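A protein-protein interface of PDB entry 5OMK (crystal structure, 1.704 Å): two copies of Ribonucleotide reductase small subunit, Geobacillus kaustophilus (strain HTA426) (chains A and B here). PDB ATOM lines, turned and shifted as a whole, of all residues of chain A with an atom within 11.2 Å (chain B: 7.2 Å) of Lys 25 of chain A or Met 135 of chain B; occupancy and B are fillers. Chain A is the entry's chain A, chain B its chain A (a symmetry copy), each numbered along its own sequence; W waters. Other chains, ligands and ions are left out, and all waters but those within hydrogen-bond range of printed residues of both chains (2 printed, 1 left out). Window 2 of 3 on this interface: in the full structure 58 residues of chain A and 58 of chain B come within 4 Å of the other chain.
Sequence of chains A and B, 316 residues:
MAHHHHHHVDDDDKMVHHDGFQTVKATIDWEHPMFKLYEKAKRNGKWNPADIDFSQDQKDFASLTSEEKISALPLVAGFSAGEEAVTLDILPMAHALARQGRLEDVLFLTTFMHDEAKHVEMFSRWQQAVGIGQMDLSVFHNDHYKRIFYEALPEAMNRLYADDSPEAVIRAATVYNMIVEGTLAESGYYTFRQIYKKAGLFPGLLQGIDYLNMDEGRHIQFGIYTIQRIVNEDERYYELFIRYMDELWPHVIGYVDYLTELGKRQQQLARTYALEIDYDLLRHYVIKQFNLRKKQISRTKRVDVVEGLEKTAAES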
ATOM      1  N   HIS A  17      26.158  32.742 -21.996  1.00  0.00           N
ATOM      2  CA  HIS A  17      25.040  32.210 -22.760  1.00  0.00           C
ATOM      3  C   HIS A  17      23.743  32.197 -21.941  1.00  0.00           C
ATOM      4  O   HIS A  17      23.736  32.373 -20.722  1.00  0.00           O
ATOM      5  CB  HIS A  17      25.386  30.793 -23.224  1.00  0.00           C
ATOM      6  CG  HIS A  17      26.581  30.730 -24.132  1.00  0.00           C
ATOM      7  ND1 HIS A  17      27.208  31.861 -24.616  1.00  0.00           N
ATOM      8  CD2 HIS A  17      27.262  29.674 -24.644  1.00  0.00           C
ATOM      9  CE1 HIS A  17      28.216  31.505 -25.391  1.00  0.00           C
ATOM     10  NE2 HIS A  17      28.271  30.185 -25.428  1.00  0.00           N
ATOM     11  N   HIS A  18      22.627  31.971 -22.644  1.00  0.00           N
ATOM     12  CA  HIS A  18      21.359  31.618 -22.011  1.00  0.00           C
ATOM     13  C   HIS A  18      21.259  30.099 -21.935  1.00  0.00           C
ATOM     14  O   HIS A  18      21.436  29.424 -22.951  1.00  0.00           O
ATOM     15  CB  HIS A  18      20.168  32.153 -22.808  1.00  0.00           C
ATOM     16  CG  HIS A  18      20.153  33.643 -22.978  1.00  0.00           C
ATOM     17  ND1 HIS A  18      19.917  34.512 -21.935  1.00  0.00           N
ATOM     18  CD2 HIS A  18      20.305  34.412 -24.085  1.00  0.00           C
ATOM     19  CE1 HIS A  18      19.945  35.756 -22.389  1.00  0.00           C
ATOM     20  NE2 HIS A  18      20.187  35.723 -23.690  1.00  0.00           N
ATOM     21  N   ASP A  19      20.975  29.557 -20.745  1.00  0.00           N
ATOM     22  CA  ASP A  19      20.793  28.107 -20.647  1.00  0.00           C
ATOM     23  C   ASP A  19      19.388  27.684 -21.079  1.00  0.00           C
ATOM     24  O   ASP A  19      19.210  26.552 -21.534  1.00  0.00           O
ATOM     25  CB  ASP A  19      21.117  27.602 -19.219  1.00  0.00           C
ATOM     26  CG  ASP A  19      22.630  27.265 -19.017  1.00  0.00           C
ATOM     27  OD1 ASP A  19      23.272  27.817 -18.088  1.00  0.00           O
ATOM     28  OD2 ASP A  19      23.185  26.441 -19.783  1.00  0.00           O
ATOM     29  N   GLY A  20      18.412  28.580 -20.994  1.00  0.00           N
ATOM     30  CA  GLY A  20      17.073  28.329 -21.503  1.00  0.00           C
ATOM     31  C   GLY A  20      16.230  29.567 -21.269  1.00  0.00           C
ATOM     32  O   GLY A  20      16.754  30.602 -20.868  1.00  0.00           O
ATOM     33  N   PHE A  21      14.913  29.456 -21.492  1.00  0.00           N
ATOM     34  CA  PHE A  21      14.011  30.603 -21.376  1.00  0.00           C
ATOM     35  C   PHE A  21      12.739  30.234 -20.620  1.00  0.00           C
ATOM     36  O   PHE A  21      12.065  29.243 -20.939  1.00  0.00           O
ATOM     37  CB  PHE A  21      13.703  31.166 -22.773  1.00  0.00           C
ATOM     38  CG  PHE A  21      14.933  31.661 -23.475  1.00  0.00           C
ATOM     39  CD1 PHE A  21      15.461  32.904 -23.157  1.00  0.00           C
ATOM     40  CD2 PHE A  21      15.606  30.866 -24.400  1.00  0.00           C
ATOM     41  CE1 PHE A  21      16.621  33.364 -23.771  1.00  0.00           C
ATOM     42  CE2 PHE A  21      16.776  31.320 -25.024  1.00  0.00           C
ATOM     43  CZ  PHE A  21      17.284  32.557 -24.713  1.00  0.00           C
ATOM     44  N   GLN A  22      12.423  31.039 -19.612  1.00  0.00           N
ATOM     45  CA  GLN A  22      11.285  30.738 -18.751  1.00  0.00           C
ATOM     46  C   GLN A  22       9.981  30.651 -19.542  1.00  0.00           C
ATOM     47  O   GLN A  22       9.124  29.814 -19.225  1.00  0.00           O
ATOM     48  CB  GLN A  22      11.184  31.789 -17.631  1.00  0.00           C
ATOM     49  CG  GLN A  22       9.988  31.604 -16.701  1.00  0.00           C
ATOM     50  CD  GLN A  22       9.950  32.652 -15.596  1.00  0.00           C
ATOM     51  OE1 GLN A  22      10.999  33.144 -15.156  1.00  0.00           O
ATOM     52  NE2 GLN A  22       8.751  33.042 -15.192  1.00  0.00           N
ATOM     53  N   THR A  23       9.792  31.509 -20.560  1.00  0.00           N
ATOM     54  CA  THR A  23       8.500  31.538 -21.252  1.00  0.00           C
ATOM     55  C   THR A  23       8.435  30.510 -22.377  1.00  0.00           C
ATOM     56  O   THR A  23       7.408  30.419 -23.066  1.00  0.00           O
ATOM     57  CB  THR A  23       8.191  32.949 -21.798  1.00  0.00           C
ATOM     58  OG1 THR A  23       9.276  33.405 -22.614  1.00  0.00           O
ATOM     59  CG2 THR A  23       7.949  33.912 -20.622  1.00  0.00           C
ATOM     60  N   VAL A  24       9.504  29.740 -22.554  1.00  0.00           N
ATOM     61  CA  VAL A  24       9.507  28.556 -23.408  1.00  0.00           C
ATOM     62  C   VAL A  24       9.305  27.285 -22.587  1.00  0.00           C
ATOM     63  O   VAL A  24       8.475  26.438 -22.928  1.00  0.00           O
ATOM     64  CB  VAL A  24      10.822  28.506 -24.206  1.00  0.00           C
ATOM     65  CG1 VAL A  24      10.981  27.176 -24.962  1.00  0.00           C
ATOM     66  CG2 VAL A  24      10.873  29.682 -25.157  1.00  0.00           C
ATOM     67  N   LYS A  25      10.060  27.152 -21.492  1.00  0.00           N
ATOM     68  CA  LYS A  25       9.895  26.024 -20.579  1.00  0.00           C
ATOM     69  C   LYS A  25       8.580  26.089 -19.830  1.00  0.00           C
ATOM     70  O   LYS A  25       8.033  25.049 -19.456  1.00  0.00           O
ATOM     71  CB  LYS A  25      11.046  25.994 -19.559  1.00  0.00           C
ATOM     72  CG  LYS A  25      12.413  25.651 -20.163  1.00  0.00           C
ATOM     73  CD  LYS A  25      13.536  26.538 -19.644  1.00  0.00           C
ATOM     74  CE  LYS A  25      14.574  25.769 -18.823  1.00  0.00           C
ATOM     75  NZ  LYS A  25      15.551  26.719 -18.161  1.00  0.00           N
ATOM     76  N   ALA A  26       8.073  27.291 -19.566  1.00  0.00           N
ATOM     77  CA  ALA A  26       6.900  27.451 -18.719  1.00  0.00           C
ATOM     78  C   ALA A  26       6.178  28.737 -19.096  1.00  0.00           C
ATOM     79  O   ALA A  26       5.880  28.939 -20.270  1.00  0.00           O
ATOM     80  CB  ALA A  26       7.304  27.428 -17.235  1.00  0.00           C
ATOM     81  N   THR A  27       5.836  29.582 -18.128  1.00  0.00           N
ATOM     82  CA  THR A  27       5.257  30.887 -18.411  1.00  0.00           C
ATOM     83  C   THR A  27       5.809  31.882 -17.398  1.00  0.00           C
ATOM     84  O   THR A  27       6.522  31.515 -16.461  1.00  0.00           O
ATOM     85  CB  THR A  27       3.725  30.895 -18.326  1.00  0.00           C
ATOM     86  OG1 THR A  27       3.318  30.757 -16.951  1.00  0.00           O
ATOM     87  CG2 THR A  27       3.094  29.757 -19.150  1.00  0.00           C
ATOM     88  N   ILE A  28       5.456  33.153 -17.595  1.00  0.00           N
ATOM     89  CA  ILE A  28       5.587  34.160 -16.547  1.00  0.00           C
ATOM     90  C   ILE A  28       4.934  33.638 -15.269  1.00  0.00           C
ATOM     91  O   ILE A  28       3.899  32.959 -15.312  1.00  0.00           O
ATOM     92  CB  ILE A  28       4.927  35.465 -17.038  1.00  0.00           C
ATOM     93  CG1 ILE A  28       5.740  36.099 -18.184  1.00  0.00           C
ATOM     94  CG2 ILE A  28       4.711  36.452 -15.917  1.00  0.00           C
ATOM     95  CD1 ILE A  28       5.022  37.282 -18.837  1.00  0.00           C
ATOM     96  N   ASP A  29       5.544  33.935 -14.120  1.00  0.00           N
ATOM     97  CA  ASP A  29       4.869  33.728 -12.834  1.00  0.00           C
ATOM     98  C   ASP A  29       3.848  34.845 -12.605  1.00  0.00           C
ATOM     99  O   ASP A  29       4.161  35.918 -12.095  1.00  0.00           O
ATOM    100  CB  ASP A  29       5.895  33.643 -11.718  1.00  0.00           C
ATOM    101  CG  ASP A  29       5.255  33.450 -10.343  1.00  0.00           C
ATOM    102  OD1 ASP A  29       4.019  33.259 -10.268  1.00  0.00           O
ATOM    103  OD2 ASP A  29       5.998  33.512  -9.340  1.00  0.00           O
ATOM    104  N   TRP A  30       2.605  34.593 -13.021  1.00  0.00           N
ATOM    105  CA  TRP A  30       1.559  35.609 -13.048  1.00  0.00           C
ATOM    106  C   TRP A  30       1.218  36.159 -11.673  1.00  0.00           C
ATOM    107  O   TRP A  30       0.662  37.267 -11.580  1.00  0.00           O
ATOM    108  CB  TRP A  30       0.284  35.028 -13.683  1.00  0.00           C
ATOM    109  CG  TRP A  30       0.517  34.324 -14.959  1.00  0.00           C
ATOM    110  CD1 TRP A  30       0.445  32.976 -15.192  1.00  0.00           C
ATOM    111  CD2 TRP A  30       0.852  34.937 -16.203  1.00  0.00           C
ATOM    112  NE1 TRP A  30       0.738  32.712 -16.508  1.00  0.00           N
ATOM    113  CE2 TRP A  30       0.981  33.906 -17.153  1.00  0.00           C
ATOM    114  CE3 TRP A  30       1.057  36.263 -16.600  1.00  0.00           C
ATOM    115  CZ2 TRP A  30       1.324  34.151 -18.491  1.00  0.00           C
ATOM    116  CZ3 TRP A  30       1.414  36.519 -17.950  1.00  0.00           C
ATOM    117  CH2 TRP A  30       1.534  35.463 -18.872  1.00  0.00           C
ATOM    118  N   GLN A 100      20.158  36.852 -12.484  1.00  0.00           N
ATOM    119  CA  GLN A 100      19.616  35.909 -11.523  1.00  0.00           C
ATOM    120  C   GLN A 100      18.350  35.235 -12.000  1.00  0.00           C
ATOM    121  O   GLN A 100      17.771  34.451 -11.240  1.00  0.00           O
ATOM    122  CB  GLN A 100      19.349  36.607 -10.193  1.00  0.00           C
ATOM    123  CG  GLN A 100      20.594  37.138  -9.507  1.00  0.00           C
ATOM    124  CD  GLN A 100      20.313  37.865  -8.231  1.00  0.00           C
ATOM    125  OE1 GLN A 100      19.177  37.990  -7.821  1.00  0.00           O
ATOM    126  NE2 GLN A 100      21.368  38.367  -7.587  1.00  0.00           N
ATOM    127  N   GLY A 101      17.886  35.496 -13.217  1.00  0.00           N
ATOM    128  CA  GLY A 101      16.690  34.806 -13.657  1.00  0.00           C
ATOM    129  C   GLY A 101      15.396  35.362 -13.119  1.00  0.00           C
ATOM    130  O   GLY A 101      14.355  34.730 -13.294  1.00  0.00           O
ATOM    131  N   LEU A 103      12.776  37.139 -13.904  1.00  0.00           N
ATOM    132  CA  LEU A 103      12.193  37.705 -15.131  1.00  0.00           C
ATOM    133  C   LEU A 103      11.103  38.719 -14.818  1.00  0.00           C
ATOM    134  O   LEU A 103      11.031  39.785 -15.446  1.00  0.00           O
ATOM    135  CB  LEU A 103      11.644  36.593 -16.027  1.00  0.00           C
ATOM    136  CG  LEU A 103      10.908  37.062 -17.298  1.00  0.00           C
ATOM    137  CD1 LEU A 103      11.839  37.746 -18.246  1.00  0.00           C
ATOM    138  CD2 LEU A 103      10.274  35.849 -17.957  1.00  0.00           C
ATOM    139  N   GLU A 104      10.256  38.426 -13.833  1.00  0.00           N
ATOM    140  CA  GLU A 104       9.185  39.366 -13.509  1.00  0.00           C
ATOM    141  C   GLU A 104       9.750  40.676 -12.975  1.00  0.00           C
ATOM    142  O   GLU A 104       9.211  41.752 -13.254  1.00  0.00           O
ATOM    143  CB  GLU A 104       8.228  38.743 -12.513  1.00  0.00           C
ATOM    144  CG  GLU A 104       7.472  37.527 -13.048  1.00  0.00           C
ATOM    145  CD  GLU A 104       8.314  36.262 -13.027  1.00  0.00           C
ATOM    146  OE1 GLU A 104       9.317  36.235 -12.284  1.00  0.00           O
ATOM    147  OE2 GLU A 104       7.981  35.311 -13.774  1.00  0.00           O
ATOM    148  N   PHE B  61      -7.545  26.523 -30.631  1.00  0.00           N
ATOM    149  CA  PHE B  61      -6.524  25.537 -30.312  1.00  0.00           C
ATOM    150  C   PHE B  61      -7.149  24.224 -29.841  1.00  0.00           C
ATOM    151  O   PHE B  61      -6.668  23.148 -30.196  1.00  0.00           O
ATOM    152  CB  PHE B  61      -5.587  26.096 -29.233  1.00  0.00           C
ATOM    153  CG  PHE B  61      -4.286  25.368 -29.135  1.00  0.00           C
ATOM    154  CD1 PHE B  61      -3.284  25.617 -30.042  1.00  0.00           C
ATOM    155  CD2 PHE B  61      -4.076  24.425 -28.151  1.00  0.00           C
ATOM    156  CE1 PHE B  61      -2.082  24.967 -29.980  1.00  0.00           C
ATOM    157  CE2 PHE B  61      -2.832  23.756 -28.076  1.00  0.00           C
ATOM    158  CZ  PHE B  61      -1.855  24.019 -29.002  1.00  0.00           C
ATOM    159  N   LYS B  69      -2.516  20.904 -33.644  1.00  0.00           N
ATOM    160  CA  LYS B  69      -2.010  21.671 -32.508  1.00  0.00           C
ATOM    161  C   LYS B  69      -0.517  21.907 -32.647  1.00  0.00           C
ATOM    162  O   LYS B  69      -0.038  23.042 -32.560  1.00  0.00           O
ATOM    163  CB  LYS B  69      -2.310  20.937 -31.188  1.00  0.00           C
ATOM    164  CG  LYS B  69      -3.738  21.027 -30.682  1.00  0.00           C
ATOM    165  CD  LYS B  69      -3.861  20.376 -29.302  1.00  0.00           C
ATOM    166  CE  LYS B  69      -5.169  20.690 -28.573  1.00  0.00           C
ATOM    167  NZ  LYS B  69      -6.352  19.950 -29.062  1.00  0.00           N
ATOM    168  N   ILE B  70       0.240  20.844 -32.896  1.00  0.00           N
ATOM    169  CA  ILE B  70       1.690  20.971 -32.879  1.00  0.00           C
ATOM    170  C   ILE B  70       2.188  21.881 -33.996  1.00  0.00           C
ATOM    171  O   ILE B  70       3.257  22.495 -33.865  1.00  0.00           O
ATOM    172  CB  ILE B  70       2.340  19.583 -32.955  1.00  0.00           C
ATOM    173  CG1 ILE B  70       3.756  19.649 -32.408  1.00  0.00           C
ATOM    174  CG2 ILE B  70       2.358  19.060 -34.396  1.00  0.00           C
ATOM    175  CD1 ILE B  70       4.273  18.322 -32.008  1.00  0.00           C
ATOM    176  N   LEU B  73       3.443  25.336 -32.861  1.00  0.00           N
ATOM    177  CA  LEU B  73       4.284  25.465 -31.677  1.00  0.00           C
ATOM    178  C   LEU B  73       5.743  25.792 -31.989  1.00  0.00           C
ATOM    179  O   LEU B  73       6.353  26.549 -31.227  1.00  0.00           O
ATOM    180  CB  LEU B  73       4.191  24.192 -30.831  1.00  0.00           C
ATOM    181  CG  LEU B  73       2.788  23.869 -30.276  1.00  0.00           C
ATOM    182  CD1 LEU B  73       2.904  22.789 -29.237  1.00  0.00           C
ATOM    183  CD2 LEU B  73       2.055  25.084 -29.691  1.00  0.00           C
ATOM    184  N   GLU B  84      12.265  36.907 -25.016  1.00  0.00           N
ATOM    185  CA  GLU B  84      12.897  36.896 -23.711  1.00  0.00           C
ATOM    186  C   GLU B  84      14.388  37.198 -23.822  1.00  0.00           C
ATOM    187  O   GLU B  84      14.921  37.997 -23.033  1.00  0.00           O
ATOM    188  CB  GLU B  84      12.622  35.545 -23.049  1.00  0.00           C
ATOM    189  CG  GLU B  84      12.948  35.480 -21.549  1.00  0.00           C
ATOM    190  CD  GLU B  84      12.503  34.144 -20.918  1.00  0.00           C
ATOM    191  OE1 GLU B  84      11.388  33.661 -21.262  1.00  0.00           O
ATOM    192  OE2 GLU B  84      13.269  33.601 -20.090  1.00  0.00           O
ATOM    193  N   GLN B 127       0.216  31.348 -24.722  1.00  0.00           N
ATOM    194  CA  GLN B 127       0.514  29.975 -24.321  1.00  0.00           C
ATOM    195  C   GLN B 127      -0.348  29.553 -23.126  1.00  0.00           C
ATOM    196  O   GLN B 127      -0.934  28.455 -23.112  1.00  0.00           O
ATOM    197  CB  GLN B 127       1.996  29.848 -23.969  1.00  0.00           C
ATOM    198  CG  GLN B 127       2.970  29.857 -25.142  1.00  0.00           C
ATOM    199  CD  GLN B 127       4.351  29.436 -24.738  1.00  0.00           C
ATOM    200  OE1 GLN B 127       4.531  28.452 -24.018  1.00  0.00           O
ATOM    201  NE2 GLN B 127       5.350  30.194 -25.162  1.00  0.00           N
ATOM    202  N   GLY B 131      -3.585  26.703 -23.252  1.00  0.00           N
ATOM    203  CA  GLY B 131      -3.381  25.499 -22.472  1.00  0.00           C
ATOM    204  C   GLY B 131      -2.050  24.815 -22.658  1.00  0.00           C
ATOM    205  O   GLY B 131      -1.939  23.632 -22.331  1.00  0.00           O
ATOM    206  N   ILE B 132      -1.039  25.501 -23.183  1.00  0.00           N
ATOM    207  CA  ILE B 132       0.273  24.894 -23.377  1.00  0.00           C
ATOM    208  C   ILE B 132       1.330  25.536 -22.504  1.00  0.00           C
ATOM    209  O   ILE B 132       2.510  25.287 -22.709  1.00  0.00           O
ATOM    210  CB  ILE B 132       0.724  24.931 -24.840  1.00  0.00           C
ATOM    211  CG1 ILE B 132       0.913  26.381 -25.332  1.00  0.00           C
ATOM    212  CG2 ILE B 132      -0.253  24.156 -25.726  1.00  0.00           C
ATOM    213  CD1 ILE B 132       1.666  26.475 -26.617  1.00  0.00           C
ATOM    214  N   GLY B 133       0.940  26.360 -21.531  1.00  0.00           N
ATOM    215  CA  GLY B 133       1.944  27.008 -20.697  1.00  0.00           C
ATOM    216  C   GLY B 133       2.846  26.009 -20.007  1.00  0.00           C
ATOM    217  O   GLY B 133       4.036  26.275 -19.789  1.00  0.00           O
ATOM    218  N   GLN B 134       2.291  24.852 -19.628  1.00  0.00           N
ATOM    219  CA  GLN B 134       3.031  23.796 -18.946  1.00  0.00           C
ATOM    220  C   GLN B 134       3.936  22.985 -19.882  1.00  0.00           C
ATOM    221  O   GLN B 134       4.804  22.257 -19.398  1.00  0.00           O
ATOM    222  CB  GLN B 134       2.028  22.878 -18.211  1.00  0.00           C
ATOM    223  CG  GLN B 134       1.221  21.917 -19.063  1.00  0.00           C
ATOM    224  CD  GLN B 134       0.183  22.533 -19.980  1.00  0.00           C
ATOM    225  OE1 GLN B 134      -0.291  23.660 -19.785  1.00  0.00           O
ATOM    226  NE2 GLN B 134      -0.195  21.769 -21.003  1.00  0.00           N
ATOM    227  N   MET B 135       3.809  23.149 -21.199  1.00  0.00           N
ATOM    228  CA  MET B 135       4.587  22.403 -22.173  1.00  0.00           C
ATOM    229  C   MET B 135       5.929  23.071 -22.429  1.00  0.00           C
ATOM    230  O   MET B 135       5.991  24.274 -22.678  1.00  0.00           O
ATOM    231  CB  MET B 135       3.777  22.303 -23.466  1.00  0.00           C
ATOM    232  CG  MET B 135       4.380  21.499 -24.590  1.00  0.00           C
ATOM    233  SD  MET B 135       3.335  21.563 -26.090  1.00  0.00           S
ATOM    234  CE  MET B 135       1.720  21.083 -25.447  1.00  0.00           C
ATOM    235  N   ASP B 136       7.002  22.288 -22.392  1.00  0.00           N
ATOM    236  CA  ASP B 136       8.347  22.818 -22.620  1.00  0.00           C
ATOM    237  C   ASP B 136       8.603  22.844 -24.120  1.00  0.00           C
ATOM    238  O   ASP B 136       8.845  21.808 -24.744  1.00  0.00           O
ATOM    239  CB  ASP B 136       9.388  21.993 -21.871  1.00  0.00           C
ATOM    240  CG  ASP B 136      10.810  22.519 -22.063  1.00  0.00           C
ATOM    241  OD1 ASP B 136      11.016  23.416 -22.907  1.00  0.00           O
ATOM    242  OD2 ASP B 136      11.725  22.031 -21.357  1.00  0.00           O
ATOM    243  N   LEU B 137       8.534  24.036 -24.712  1.00  0.00           N
ATOM    244  CA  LEU B 137       8.661  24.174 -26.154  1.00  0.00           C
ATOM    245  C   LEU B 137      10.114  24.278 -26.614  1.00  0.00           C
ATOM    246  O   LEU B 137      10.347  24.521 -27.797  1.00  0.00           O
ATOM    247  CB  LEU B 137       7.865  25.391 -26.638  1.00  0.00           C
ATOM    248  CG  LEU B 137       6.383  25.426 -26.252  1.00  0.00           C
ATOM    249  CD1 LEU B 137       5.715  26.667 -26.857  1.00  0.00           C
ATOM    250  CD2 LEU B 137       5.662  24.211 -26.708  1.00  0.00           C
ATOM    251  N   SER B 138      11.092  24.050 -25.716  1.00  0.00           N
ATOM    252  CA  SER B 138      12.510  24.078 -26.082  1.00  0.00           C
ATOM    253  C   SER B 138      12.878  23.007 -27.098  1.00  0.00           C
ATOM    254  O   SER B 138      13.905  23.135 -27.783  1.00  0.00           O
ATOM    255  CB  SER B 138      13.410  23.876 -24.841  1.00  0.00           C
ATOM    256  OG  SER B 138      13.170  24.843 -23.831  1.00  0.00           O
ATOM    257  N   VAL B 139      12.092  21.931 -27.178  1.00  0.00           N
ATOM    258  CA  VAL B 139      12.331  20.889 -28.172  1.00  0.00           C
ATOM    259  C   VAL B 139      12.364  21.418 -29.606  1.00  0.00           C
ATOM    260  O   VAL B 139      12.948  20.770 -30.488  1.00  0.00           O
ATOM    261  CB  VAL B 139      11.283  19.756 -28.033  1.00  0.00           C
ATOM    262  CG1 VAL B 139       9.857  20.278 -28.195  1.00  0.00           C
ATOM    263  CG2 VAL B 139      11.564  18.660 -29.062  1.00  0.00           C
ATOM    264  N   PHE B 140      11.807  22.597 -29.870  1.00  0.00           N
ATOM    265  CA  PHE B 140      11.784  23.127 -31.230  1.00  0.00           C
ATOM    266  C   PHE B 140      12.898  24.134 -31.497  1.00  0.00           C
ATOM    267  O   PHE B 140      12.861  24.829 -32.513  1.00  0.00           O
ATOM    268  CB  PHE B 140      10.432  23.769 -31.535  1.00  0.00           C
ATOM    269  CG  PHE B 140       9.282  22.830 -31.403  1.00  0.00           C
ATOM    270  CD1 PHE B 140       9.176  21.705 -32.220  1.00  0.00           C
ATOM    271  CD2 PHE B 140       8.299  23.063 -30.465  1.00  0.00           C
ATOM    272  CE1 PHE B 140       8.101  20.834 -32.083  1.00  0.00           C
ATOM    273  CE2 PHE B 140       7.221  22.187 -30.332  1.00  0.00           C
ATOM    274  CZ  PHE B 140       7.134  21.075 -31.142  1.00  0.00           C
ATOM    275  N   HIS B 141      13.899  24.196 -30.636  1.00  0.00           N
ATOM    276  CA  HIS B 141      15.091  24.995 -30.871  1.00  0.00           C
ATOM    277  C   HIS B 141      16.200  24.068 -31.349  1.00  0.00           C
ATOM    278  O   HIS B 141      16.796  23.353 -30.543  1.00  0.00           O
ATOM    279  CB  HIS B 141      15.534  25.716 -29.595  1.00  0.00           C
ATOM    280  CG  HIS B 141      14.548  26.716 -29.085  1.00  0.00           C
ATOM    281  ND1 HIS B 141      14.586  27.210 -27.795  1.00  0.00           N
ATOM    282  CD2 HIS B 141      13.502  27.320 -29.690  1.00  0.00           C
ATOM    283  CE1 HIS B 141      13.596  28.061 -27.623  1.00  0.00           C
ATOM    284  NE2 HIS B 141      12.928  28.157 -28.763  1.00  0.00           N
ATOM    285  N   TYR B 150      20.871  31.457 -27.985  1.00  0.00           N
ATOM    286  CA  TYR B 150      21.473  31.075 -26.711  1.00  0.00           C
ATOM    287  C   TYR B 150      22.913  31.549 -26.594  1.00  0.00           C
ATOM    288  O   TYR B 150      23.408  31.713 -25.474  1.00  0.00           O
ATOM    289  CB  TYR B 150      21.457  29.561 -26.508  1.00  0.00           C
ATOM    290  CG  TYR B 150      20.091  28.890 -26.333  1.00  0.00           C
ATOM    291  CD1 TYR B 150      19.921  27.912 -25.352  1.00  0.00           C
ATOM    292  CD2 TYR B 150      19.006  29.180 -27.159  1.00  0.00           C
ATOM    293  CE1 TYR B 150      18.726  27.255 -25.190  1.00  0.00           C
ATOM    294  CE2 TYR B 150      17.773  28.523 -26.995  1.00  0.00           C
ATOM    295  CZ  TYR B 150      17.650  27.552 -26.003  1.00  0.00           C
ATOM    296  OH  TYR B 150      16.482  26.853 -25.787  1.00  0.00           O
HETATM  297  O   HOH W   1       5.097  31.067 -21.820  1.00  0.00           O
HETATM  298  O   HOH W   2      14.393  27.192 -23.498  1.00  0.00           O
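O of Tyr 150 of chain B sits at hydrogen-bond distance from N of His 18 of chain A. N of Gln 22 of chain A sits at hydrogen-bond distance from OE2 of Glu 84 of chain B (2.7 Å). The side-chain carboxylate of Glu 84 of chain B sits at hydrogen-bond distance from the side-chain hydroxyl of Thr 23 of chain A (2.5 Å). The backbone carbonyl oxygen (O) of Thr 23 of chain A is in hydrogen-bond range of the side-chain amide nitrogen (NE2) of Gln 127 of chain B. The backbone carbonyl oxygen (O) of Val 24 of chain A sits at hydrogen-bond distance from the backbone NH (N) of Leu 137 of chain B (3.0 Å). The backbone carbonyl oxygen (O) of Val 24 of chain A sits close to the backbone carbonyl oxygen (O) of Met 135 of chain B, 3.3 Å away. O of Gly 133 of chain B lies close to O of Ala 26 of chain A, at 3.3 Å.
NE2 of Gln 22 of chain A is in hydrogen-bond range of O of Thr 27 of chain A, 3.0 Å away. The side-chain hydroxyl of Thr 27 of chain A lies within hydrogen-bond range of the indole nitrogen of Trp 30 of chain A. The side-chain hydroxyl (OH) of Tyr 150 of chain B is in hydrogen-bond range of a ring nitrogen (ND1) of His 141 of chain B, 2.8 Å away.
Among the printed residues, merely in contact across the chains: His 17 of chain A with Tyr 150 of chain B, Asp 19 of chain A with Tyr 150 of chain B, Phe 21 of chain A with Glu 84 of chain B, Phe 21 of chain A with Tyr 150 of chain B, Val 24 of chain A with Asp 136 of chain B, Val 24 of chain A with Ser 138 of chain B, Val 24 of chain A with His 141 of chain B, Lys 25 of chain A with Met 135 of chain B, Lys 25 of chain A with Asp 136 of chain B, Lys 25 of chain A with Ser 138 of chain B and Thr 27 of chain A with Gly 133 of chain B.
Lys 25 of chain A touches just these residues of chain B: Met 135 (3.9 Å), Asp 136 (3.7 Å) and Ser 138 (3.8 Å). Of chain A, only Val 24 and Lys 25 come within 4 Å of Met 135 of chain B. No residue of chain A comes within 4 Å of Gln 134 of chain B. Of the printed residues of chain B, Phe 21 of chain A touches Glu 84 and Tyr 150. Of the printed residues of chain A, Glu 84 of chain B touches Phe 21 (3.3 Å), Gln 22 (2.7 Å) and Thr 23 (2.5 Å). Printed residues of chain B within 4 Å of Gln 22 of chain A: Glu 84. Leu 73 of chain B touches none of the printed residues of chain A. The nearest residue of chain B that does not touch Lys 25 of chain A is Gly 133 of chain B (4.2 Å). The nearest residue of chain A that does not touch Met 135 of chain B is Ala 26 of chain A (4.8 Å). The nearest printed residue of chain B that does not touch Thr 23 of chain A is Leu 137 of chain B (5.6 Å).
Of the 18 printed residues of chain B, 9 touch a printed residue of chain A. Among the printed residues, 18 pairs touch across the chains. Among the printed residues, no Asp or Glu carboxylate lies within 4 Å of a Lys or Arg side-chain nitrogen of the other chain.
No position is printed for both chains. Of the 18 pairs that touch across the chains among the printed residues, none has its exchanged pair printed and touching as well.
Water W2 lies within hydrogen-bond range of OG of Ser 138 of chain B (2.7 Å), N of Phe 21 of chain A (3.1 Å) and OH of Tyr 150 of chain B (3.1 Å).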
